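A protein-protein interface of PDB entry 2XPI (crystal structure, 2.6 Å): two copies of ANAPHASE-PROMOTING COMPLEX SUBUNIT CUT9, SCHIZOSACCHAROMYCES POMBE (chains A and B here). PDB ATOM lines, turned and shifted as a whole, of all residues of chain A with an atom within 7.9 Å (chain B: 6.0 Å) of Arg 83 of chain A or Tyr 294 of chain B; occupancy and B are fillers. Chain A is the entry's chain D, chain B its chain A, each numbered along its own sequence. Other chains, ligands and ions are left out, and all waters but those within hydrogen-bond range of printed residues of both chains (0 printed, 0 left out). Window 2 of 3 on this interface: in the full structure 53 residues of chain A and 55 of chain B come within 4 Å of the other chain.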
ATOM      1  N   LEU A  81      -3.930 -13.348  33.927  1.00  0.00           N
ATOM      2  CA  LEU A  81      -3.292 -12.034  33.774  1.00  0.00           C
ATOM      3  C   LEU A  81      -3.592 -11.406  32.435  1.00  0.00           C
ATOM      4  O   LEU A  81      -3.587 -12.075  31.420  1.00  0.00           O
ATOM      5  CB  LEU A  81      -1.778 -12.105  33.985  1.00  0.00           C
ATOM      6  CG  LEU A  81      -1.348 -12.052  35.462  1.00  0.00           C
ATOM      7  CD1 LEU A  81      -1.980 -13.175  36.259  1.00  0.00           C
ATOM      8  CD2 LEU A  81       0.174 -12.100  35.573  1.00  0.00           C
ATOM      9  N   SER A  82      -3.853 -10.111  32.426  1.00  0.00           N
ATOM     10  CA  SER A  82      -4.185  -9.449  31.185  1.00  0.00           C
ATOM     11  C   SER A  82      -2.905  -9.231  30.352  1.00  0.00           C
ATOM     12  O   SER A  82      -1.790  -9.500  30.803  1.00  0.00           O
ATOM     13  CB  SER A  82      -4.887  -8.121  31.479  1.00  0.00           C
ATOM     14  OG  SER A  82      -3.999  -7.190  32.087  1.00  0.00           O
ATOM     15  N   ARG A  83      -3.058  -8.736  29.135  1.00  0.00           N
ATOM     16  CA  ARG A  83      -1.892  -8.414  28.328  1.00  0.00           C
ATOM     17  C   ARG A  83      -1.069  -7.303  28.978  1.00  0.00           C
ATOM     18  O   ARG A  83       0.161  -7.332  28.965  1.00  0.00           O
ATOM     19  CB  ARG A  83      -2.329  -8.003  26.931  1.00  0.00           C
ATOM     20  CG  ARG A  83      -1.329  -7.176  26.207  1.00  0.00           C
ATOM     21  CD  ARG A  83      -1.370  -7.549  24.766  1.00  0.00           C
ATOM     22  NE  ARG A  83      -2.454  -6.892  24.057  1.00  0.00           N
ATOM     23  CZ  ARG A  83      -3.261  -7.497  23.196  1.00  0.00           C
ATOM     24  NH1 ARG A  83      -3.140  -8.797  22.949  1.00  0.00           N
ATOM     25  NH2 ARG A  83      -4.189  -6.784  22.587  1.00  0.00           N
ATOM     26  N   GLU A  84      -1.750  -6.321  29.554  1.00  0.00           N
ATOM     27  CA  GLU A  84      -1.044  -5.210  30.180  1.00  0.00           C
ATOM     28  C   GLU A  84      -0.386  -5.607  31.508  1.00  0.00           C
ATOM     29  O   GLU A  84       0.588  -4.973  31.917  1.00  0.00           O
ATOM     30  CB  GLU A  84      -1.964  -4.005  30.349  1.00  0.00           C
ATOM     31  CG  GLU A  84      -2.573  -3.524  29.029  1.00  0.00           C
ATOM     32  CD  GLU A  84      -3.882  -4.233  28.682  1.00  0.00           C
ATOM     33  OE1 GLU A  84      -4.287  -4.201  27.493  1.00  0.00           O
ATOM     34  OE2 GLU A  84      -4.507  -4.816  29.601  1.00  0.00           O
ATOM     35  N   ASP A  85      -0.905  -6.649  32.166  1.00  0.00           N
ATOM     36  CA  ASP A  85      -0.218  -7.239  33.312  1.00  0.00           C
ATOM     37  C   ASP A  85       1.106  -7.877  32.865  1.00  0.00           C
ATOM     38  O   ASP A  85       2.173  -7.578  33.406  1.00  0.00           O
ATOM     39  CB  ASP A  85      -1.072  -8.316  33.985  1.00  0.00           C
ATOM     40  CG  ASP A  85      -2.371  -7.772  34.594  1.00  0.00           C
ATOM     41  OD1 ASP A  85      -3.363  -8.525  34.592  1.00  0.00           O
ATOM     42  OD2 ASP A  85      -2.408  -6.622  35.083  1.00  0.00           O
ATOM     43  N   TYR A  86       1.037  -8.754  31.869  1.00  0.00           N
ATOM     44  CA  TYR A  86       2.225  -9.427  31.356  1.00  0.00           C
ATOM     45  C   TYR A  86       3.318  -8.471  30.930  1.00  0.00           C
ATOM     46  O   TYR A  86       4.495  -8.714  31.205  1.00  0.00           O
ATOM     47  CB  TYR A  86       1.874 -10.298  30.165  1.00  0.00           C
ATOM     48  CG  TYR A  86       1.343 -11.642  30.540  1.00  0.00           C
ATOM     49  CD1 TYR A  86       0.104 -12.074  30.090  1.00  0.00           C
ATOM     50  CD2 TYR A  86       2.076 -12.486  31.351  1.00  0.00           C
ATOM     51  CE1 TYR A  86      -0.380 -13.324  30.436  1.00  0.00           C
ATOM     52  CE2 TYR A  86       1.598 -13.724  31.707  1.00  0.00           C
ATOM     53  CZ  TYR A  86       0.380 -14.144  31.246  1.00  0.00           C
ATOM     54  OH  TYR A  86      -0.073 -15.390  31.596  1.00  0.00           O
ATOM     55  N   LEU A  87       2.927  -7.406  30.232  1.00  0.00           N
ATOM     56  CA  LEU A  87       3.872  -6.412  29.733  1.00  0.00           C
ATOM     57  C   LEU A  87       4.548  -5.641  30.869  1.00  0.00           C
ATOM     58  O   LEU A  87       5.745  -5.333  30.805  1.00  0.00           O
ATOM     59  CB  LEU A  87       3.160  -5.439  28.788  1.00  0.00           C
ATOM     60  CG  LEU A  87       2.613  -6.053  27.491  1.00  0.00           C
ATOM     61  CD1 LEU A  87       1.833  -5.021  26.688  1.00  0.00           C
ATOM     62  CD2 LEU A  87       3.738  -6.660  26.658  1.00  0.00           C
ATOM     63  N   ARG A  88       3.766  -5.345  31.911  1.00  0.00           N
ATOM     64  CA  ARG A  88       4.272  -4.672  33.102  1.00  0.00           C
ATOM     65  C   ARG A  88       5.239  -5.527  33.891  1.00  0.00           C
ATOM     66  O   ARG A  88       6.271  -5.039  34.305  1.00  0.00           O
ATOM     67  CB  ARG A  88       3.132  -4.237  34.005  1.00  0.00           C
ATOM     68  CG  ARG A  88       2.281  -3.148  33.424  1.00  0.00           C
ATOM     69  CD  ARG A  88       1.301  -2.673  34.449  1.00  0.00           C
ATOM     70  NE  ARG A  88       0.512  -1.579  33.918  1.00  0.00           N
ATOM     71  CZ  ARG A  88      -0.806  -1.620  33.752  1.00  0.00           C
ATOM     72  NH1 ARG A  88      -1.506  -2.701  34.090  1.00  0.00           N
ATOM     73  NH2 ARG A  88      -1.421  -0.566  33.253  1.00  0.00           N
ATOM     74  N   LEU A  89       4.908  -6.791  34.112  1.00  0.00           N
ATOM     75  CA  LEU A  89       5.832  -7.702  34.780  1.00  0.00           C
ATOM     76  C   LEU A  89       7.130  -7.768  33.966  1.00  0.00           C
ATOM     77  O   LEU A  89       8.243  -7.714  34.496  1.00  0.00           O
ATOM     78  CB  LEU A  89       5.210  -9.102  34.922  1.00  0.00           C
ATOM     79  CG  LEU A  89       4.460  -9.468  36.230  1.00  0.00           C
ATOM     80  CD1 LEU A  89       4.445  -8.370  37.310  1.00  0.00           C
ATOM     81  CD2 LEU A  89       3.083  -9.959  35.974  1.00  0.00           C
ATOM     82  N   TRP A  90       6.966  -7.848  32.657  1.00  0.00           N
ATOM     83  CA  TRP A  90       8.087  -7.953  31.753  1.00  0.00           C
ATOM     84  C   TRP A  90       8.971  -6.687  31.778  1.00  0.00           C
ATOM     85  O   TRP A  90      10.188  -6.772  31.963  1.00  0.00           O
ATOM     86  CB  TRP A  90       7.544  -8.254  30.369  1.00  0.00           C
ATOM     87  CG  TRP A  90       8.550  -8.271  29.302  1.00  0.00           C
ATOM     88  CD1 TRP A  90       9.897  -8.200  29.444  1.00  0.00           C
ATOM     89  CD2 TRP A  90       8.293  -8.358  27.908  1.00  0.00           C
ATOM     90  NE1 TRP A  90      10.506  -8.258  28.229  1.00  0.00           N
ATOM     91  CE2 TRP A  90       9.542  -8.350  27.258  1.00  0.00           C
ATOM     92  CE3 TRP A  90       7.123  -8.461  27.140  1.00  0.00           C
ATOM     93  CZ2 TRP A  90       9.663  -8.426  25.861  1.00  0.00           C
ATOM     94  CZ3 TRP A  90       7.240  -8.548  25.769  1.00  0.00           C
ATOM     95  CH2 TRP A  90       8.505  -8.528  25.141  1.00  0.00           C
ATOM     96  N   VAL A 106       9.068  -2.425  25.758  1.00  0.00           N
ATOM     97  CA  VAL A 106       7.876  -2.895  26.457  1.00  0.00           C
ATOM     98  C   VAL A 106       7.168  -1.737  27.155  1.00  0.00           C
ATOM     99  O   VAL A 106       5.939  -1.656  27.163  1.00  0.00           O
ATOM    100  CB  VAL A 106       8.243  -3.928  27.513  1.00  0.00           C
ATOM    101  CG1 VAL A 106       7.001  -4.499  28.136  1.00  0.00           C
ATOM    102  CG2 VAL A 106       9.034  -5.027  26.882  1.00  0.00           C
ATOM    103  N   VAL A 110       3.126  -0.662  26.556  1.00  0.00           N
ATOM    104  CA  VAL A 110       2.089  -0.608  27.583  1.00  0.00           C
ATOM    105  C   VAL A 110       1.510   0.796  27.729  1.00  0.00           C
ATOM    106  O   VAL A 110       0.288   0.968  27.888  1.00  0.00           O
ATOM    107  CB  VAL A 110       2.567  -1.019  28.999  1.00  0.00           C
ATOM    108  CG1 VAL A 110       1.350  -1.299  29.864  1.00  0.00           C
ATOM    109  CG2 VAL A 110       3.450  -2.234  28.963  1.00  0.00           C
ATOM    110  N   ILE A 113      -0.924   1.687  24.979  1.00  0.00           N
ATOM    111  CA  ILE A 113      -2.201   1.028  25.121  1.00  0.00           C
ATOM    112  C   ILE A 113      -3.060   1.628  26.235  1.00  0.00           C
ATOM    113  O   ILE A 113      -4.258   1.809  26.055  1.00  0.00           O
ATOM    114  CB  ILE A 113      -2.012  -0.447  25.401  1.00  0.00           C
ATOM    115  CG1 ILE A 113      -1.355  -1.119  24.205  1.00  0.00           C
ATOM    116  CG2 ILE A 113      -3.328  -1.075  25.713  1.00  0.00           C
ATOM    117  CD1 ILE A 113      -1.139  -2.574  24.417  1.00  0.00           C
ATOM    118  N   THR A 114      -2.451   1.952  27.375  1.00  0.00           N
ATOM    119  CA  THR A 114      -3.213   2.356  28.556  1.00  0.00           C
ATOM    120  C   THR A 114      -3.306   3.860  28.813  1.00  0.00           C
ATOM    121  O   THR A 114      -4.331   4.345  29.293  1.00  0.00           O
ATOM    122  CB  THR A 114      -2.635   1.734  29.834  1.00  0.00           C
ATOM    123  OG1 THR A 114      -1.408   2.389  30.156  1.00  0.00           O
ATOM    124  CG2 THR A 114      -2.403   0.244  29.659  1.00  0.00           C
ATOM    125  N   TYR B 263       6.229 -15.844  26.583  1.00  0.00           N
ATOM    126  CA  TYR B 263       5.541 -14.575  26.858  1.00  0.00           C
ATOM    127  C   TYR B 263       4.154 -14.866  27.408  1.00  0.00           C
ATOM    128  O   TYR B 263       3.874 -14.579  28.566  1.00  0.00           O
ATOM    129  CB  TYR B 263       5.432 -13.700  25.611  1.00  0.00           C
ATOM    130  CG  TYR B 263       4.353 -12.627  25.674  1.00  0.00           C
ATOM    131  CD1 TYR B 263       4.412 -11.584  26.603  1.00  0.00           C
ATOM    132  CD2 TYR B 263       3.284 -12.643  24.787  1.00  0.00           C
ATOM    133  CE1 TYR B 263       3.425 -10.589  26.644  1.00  0.00           C
ATOM    134  CE2 TYR B 263       2.303 -11.671  24.821  1.00  0.00           C
ATOM    135  CZ  TYR B 263       2.379 -10.648  25.746  1.00  0.00           C
ATOM    136  OH  TYR B 263       1.388  -9.699  25.759  1.00  0.00           O
ATOM    137  N   ASP B 267      -1.648 -15.056  24.116  1.00  0.00           N
ATOM    138  CA  ASP B 267      -1.486 -13.776  23.426  1.00  0.00           C
ATOM    139  C   ASP B 267      -0.222 -13.803  22.547  1.00  0.00           C
ATOM    140  O   ASP B 267       0.440 -12.786  22.347  1.00  0.00           O
ATOM    141  CB  ASP B 267      -1.413 -12.636  24.454  1.00  0.00           C
ATOM    142  CG  ASP B 267      -1.587 -11.267  23.830  1.00  0.00           C
ATOM    143  OD1 ASP B 267      -0.846 -10.344  24.235  1.00  0.00           O
ATOM    144  OD2 ASP B 267      -2.451 -11.118  22.934  1.00  0.00           O
ATOM    145  N   ALA B 269       0.299 -14.052  19.429  1.00  0.00           N
ATOM    146  CA  ALA B 269       0.292 -13.331  18.166  1.00  0.00           C
ATOM    147  C   ALA B 269       0.644 -11.873  18.330  1.00  0.00           C
ATOM    148  O   ALA B 269       1.152 -11.252  17.406  1.00  0.00           O
ATOM    149  CB  ALA B 269      -1.040 -13.468  17.451  1.00  0.00           C
ATOM    150  N   PHE B 270       0.362 -11.322  19.495  1.00  0.00           N
ATOM    151  CA  PHE B 270       0.656  -9.926  19.762  1.00  0.00           C
ATOM    152  C   PHE B 270       2.160  -9.693  19.763  1.00  0.00           C
ATOM    153  O   PHE B 270       2.661  -8.814  19.061  1.00  0.00           O
ATOM    154  CB  PHE B 270       0.048  -9.526  21.101  1.00  0.00           C
ATOM    155  CG  PHE B 270       0.451  -8.162  21.582  1.00  0.00           C
ATOM    156  CD1 PHE B 270      -0.153  -7.023  21.072  1.00  0.00           C
ATOM    157  CD2 PHE B 270       1.391  -8.022  22.586  1.00  0.00           C
ATOM    158  CE1 PHE B 270       0.203  -5.766  21.531  1.00  0.00           C
ATOM    159  CE2 PHE B 270       1.743  -6.782  23.048  1.00  0.00           C
ATOM    160  CZ  PHE B 270       1.144  -5.650  22.519  1.00  0.00           C
ATOM    161  N   SER B 273       3.764 -10.394  16.275  1.00  0.00           N
ATOM    162  CA  SER B 273       3.518  -9.291  15.334  1.00  0.00           C
ATOM    163  C   SER B 273       4.438  -8.103  15.623  1.00  0.00           C
ATOM    164  O   SER B 273       4.922  -7.444  14.708  1.00  0.00           O
ATOM    165  CB  SER B 273       2.051  -8.822  15.362  1.00  0.00           C
ATOM    166  OG  SER B 273       1.115  -9.881  15.171  1.00  0.00           O
ATOM    167  N   ARG B 289       1.549  -8.158   6.642  1.00  0.00           N
ATOM    168  CA  ARG B 289       0.376  -7.311   6.432  1.00  0.00           C
ATOM    169  C   ARG B 289      -0.737  -7.622   7.417  1.00  0.00           C
ATOM    170  O   ARG B 289      -1.567  -6.765   7.702  1.00  0.00           O
ATOM    171  CB  ARG B 289      -0.163  -7.436   5.005  1.00  0.00           C
ATOM    172  CG  ARG B 289      -0.820  -8.782   4.698  1.00  0.00           C
ATOM    173  CD  ARG B 289      -1.708  -8.726   3.447  1.00  0.00           C
ATOM    174  NE  ARG B 289      -2.152 -10.053   3.017  1.00  0.00           N
ATOM    175  CZ  ARG B 289      -2.925 -10.866   3.737  1.00  0.00           C
ATOM    176  NH1 ARG B 289      -3.339 -10.500   4.943  1.00  0.00           N
ATOM    177  NH2 ARG B 289      -3.275 -12.053   3.254  1.00  0.00           N
ATOM    178  N   ARG B 290      -0.766  -8.848   7.926  1.00  0.00           N
ATOM    179  CA  ARG B 290      -1.760  -9.207   8.927  1.00  0.00           C
ATOM    180  C   ARG B 290      -1.274  -8.852  10.324  1.00  0.00           C
ATOM    181  O   ARG B 290      -2.072  -8.600  11.223  1.00  0.00           O
ATOM    182  CB  ARG B 290      -2.120 -10.687   8.843  1.00  0.00           C
ATOM    183  CG  ARG B 290      -0.939 -11.606   8.689  1.00  0.00           C
ATOM    184  CD  ARG B 290      -1.394 -13.045   8.824  1.00  0.00           C
ATOM    185  NE  ARG B 290      -0.444 -13.966   8.214  1.00  0.00           N
ATOM    186  CZ  ARG B 290      -0.327 -14.151   6.903  1.00  0.00           C
ATOM    187  NH1 ARG B 290      -1.097 -13.470   6.059  1.00  0.00           N
ATOM    188  NH2 ARG B 290       0.563 -15.013   6.434  1.00  0.00           N
ATOM    189  N   ALA B 291       0.043  -8.843  10.492  1.00  0.00           N
ATOM    190  CA  ALA B 291       0.659  -8.402  11.729  1.00  0.00           C
ATOM    191  C   ALA B 291       0.385  -6.931  11.891  1.00  0.00           C
ATOM    192  O   ALA B 291       0.078  -6.460  12.986  1.00  0.00           O
ATOM    193  CB  ALA B 291       2.139  -8.632  11.685  1.00  0.00           C
ATOM    194  N   GLU B 292       0.509  -6.207  10.786  1.00  0.00           N
ATOM    195  CA  GLU B 292       0.265  -4.775  10.767  1.00  0.00           C
ATOM    196  C   GLU B 292      -1.234  -4.500  10.936  1.00  0.00           C
ATOM    197  O   GLU B 292      -1.634  -3.479  11.504  1.00  0.00           O
ATOM    198  CB  GLU B 292       0.802  -4.166   9.468  1.00  0.00           C
ATOM    199  CG  GLU B 292       0.935  -2.643   9.475  1.00  0.00           C
ATOM    200  CD  GLU B 292      -0.416  -1.920   9.397  1.00  0.00           C
ATOM    201  OE1 GLU B 292      -1.284  -2.332   8.585  1.00  0.00           O
ATOM    202  OE2 GLU B 292      -0.613  -0.938  10.151  1.00  0.00           O
ATOM    203  N   ASP B 293      -2.067  -5.418  10.460  1.00  0.00           N
ATOM    204  CA  ASP B 293      -3.495  -5.237  10.618  1.00  0.00           C
ATOM    205  C   ASP B 293      -3.945  -5.563  12.039  1.00  0.00           C
ATOM    206  O   ASP B 293      -4.671  -4.790  12.672  1.00  0.00           O
ATOM    207  CB  ASP B 293      -4.265  -6.072   9.605  1.00  0.00           C
ATOM    208  CG  ASP B 293      -5.302  -5.256   8.873  1.00  0.00           C
ATOM    209  OD1 ASP B 293      -5.044  -4.048   8.654  1.00  0.00           O
ATOM    210  OD2 ASP B 293      -6.370  -5.811   8.524  1.00  0.00           O
ATOM    211  N   TYR B 294      -3.504  -6.714  12.534  1.00  0.00           N
ATOM    212  CA  TYR B 294      -3.782  -7.114  13.899  1.00  0.00           C
ATOM    213  C   TYR B 294      -3.424  -6.000  14.886  1.00  0.00           C
ATOM    214  O   TYR B 294      -4.232  -5.650  15.746  1.00  0.00           O
ATOM    215  CB  TYR B 294      -3.019  -8.386  14.233  1.00  0.00           C
ATOM    216  CG  TYR B 294      -3.258  -8.898  15.623  1.00  0.00           C
ATOM    217  CD1 TYR B 294      -4.538  -9.222  16.058  1.00  0.00           C
ATOM    218  CD2 TYR B 294      -2.203  -9.069  16.506  1.00  0.00           C
ATOM    219  CE1 TYR B 294      -4.758  -9.709  17.344  1.00  0.00           C
ATOM    220  CE2 TYR B 294      -2.407  -9.548  17.779  1.00  0.00           C
ATOM    221  CZ  TYR B 294      -3.683  -9.867  18.197  1.00  0.00           C
ATOM    222  OH  TYR B 294      -3.874 -10.347  19.472  1.00  0.00           O
ATOM    223  N   LEU B 295      -2.229  -5.435  14.755  1.00  0.00           N
ATOM    224  CA  LEU B 295      -1.773  -4.403  15.689  1.00  0.00           C
ATOM    225  C   LEU B 295      -2.508  -3.060  15.558  1.00  0.00           C
ATOM    226  O   LEU B 295      -2.667  -2.328  16.542  1.00  0.00           O
ATOM    227  CB  LEU B 295      -0.262  -4.198  15.567  1.00  0.00           C
ATOM    228  CG  LEU B 295       0.661  -5.021  16.469  1.00  0.00           C
ATOM    229  CD1 LEU B 295      -0.086  -6.057  17.295  1.00  0.00           C
ATOM    230  CD2 LEU B 295       1.742  -5.658  15.638  1.00  0.00           C
ATOM    231  N   SER B 296      -2.956  -2.737  14.350  1.00  0.00           N
ATOM    232  CA  SER B 296      -3.766  -1.541  14.142  1.00  0.00           C
ATOM    233  C   SER B 296      -5.184  -1.687  14.710  1.00  0.00           C
ATOM    234  O   SER B 296      -5.830  -0.691  15.044  1.00  0.00           O
ATOM    235  CB  SER B 296      -3.802  -1.155  12.663  1.00  0.00           C
ATOM    236  OG  SER B 296      -2.627  -0.431  12.312  1.00  0.00           O
ATOM    237  N   SER B 297      -5.659  -2.923  14.832  1.00  0.00           N
ATOM    238  CA  SER B 297      -6.947  -3.172  15.468  1.00  0.00           C
ATOM    239  C   SER B 297      -6.863  -3.077  17.004  1.00  0.00           C
ATOM    240  O   SER B 297      -7.889  -3.001  17.684  1.00  0.00           O
ATOM    241  CB  SER B 297      -7.520  -4.534  15.045  1.00  0.00           C
ATOM    242  OG  SER B 297      -6.894  -5.606  15.730  1.00  0.00           O
ATOM    243  N   ILE B 298      -5.644  -3.092  17.541  1.00  0.00           N
ATOM    244  CA  ILE B 298      -5.440  -2.904  18.970  1.00  0.00           C
ATOM    245  C   ILE B 298      -5.534  -1.416  19.284  1.00  0.00           C
ATOM    246  O   ILE B 298      -4.756  -0.598  18.780  1.00  0.00           O
ATOM    247  CB  ILE B 298      -4.064  -3.420  19.448  1.00  0.00           C
ATOM    248  CG1 ILE B 298      -3.803  -4.838  18.953  1.00  0.00           C
ATOM    249  CG2 ILE B 298      -3.970  -3.362  20.965  1.00  0.00           C
ATOM    250  CD1 ILE B 298      -4.659  -5.865  19.606  1.00  0.00           C
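NH1 of Arg 83 of chain A is in salt-bridge range of OD2 of Asp 267 of chain B.
OH of Tyr 263 of chain B sits at hydrogen-bond distance from OD1 of Asp 267 of chain B (2.8 Å). OG of Ser 297 of chain B lies within hydrogen-bond range of O of Tyr 294 of chain B (2.7 Å).
Among the printed residues, merely in contact across the chains: Arg 83 of chain A with Ile 298 of chain B, Arg 83 of chain A with Phe 270 of chain B, Arg 83 of chain A with Tyr 263 of chain B, Tyr 86 of chain A with Tyr 263 of chain B, Arg 83 of chain A with Tyr 294 of chain B and Leu 87 of chain A with Tyr 263 of chain B.
Arg 83 of chain A touches five residues of chain B. Of the printed residues of chain A, Tyr 263 of chain B touches Arg 83 (3.6 Å), Tyr 86 (3.9 Å) and Leu 87 (3.9 Å). Printed residues of chain A within 4 Å of Asp 267 of chain B: Arg 83. Of the printed residues of chain B, Tyr 86 of chain A touches Tyr 263 (3.9 Å). Of the printed residues of chain A, Phe 270 of chain B touches Arg 83 (3.5 Å). Ala 291 of chain B touches none of the printed residues of chain A. The nearest printed residue of chain B that does not touch Arg 83 of chain A is Ala 269 of chain B (6.7 Å). The nearest printed residue of chain A that does not touch Tyr 294 of chain B is Ile 113 of chain A (9.6 Å).
Of the 14 printed residues of chain A, 3 touch a printed residue of chain B. Of the 15 printed residues of chain B, 5 touch a printed residue of chain A. Among the printed residues, 7 pairs touch across the chains.
No position is printed for both chains. Of the 7 pairs that touch across the chains among the printed residues, none has its exchanged pair printed and touching as well.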
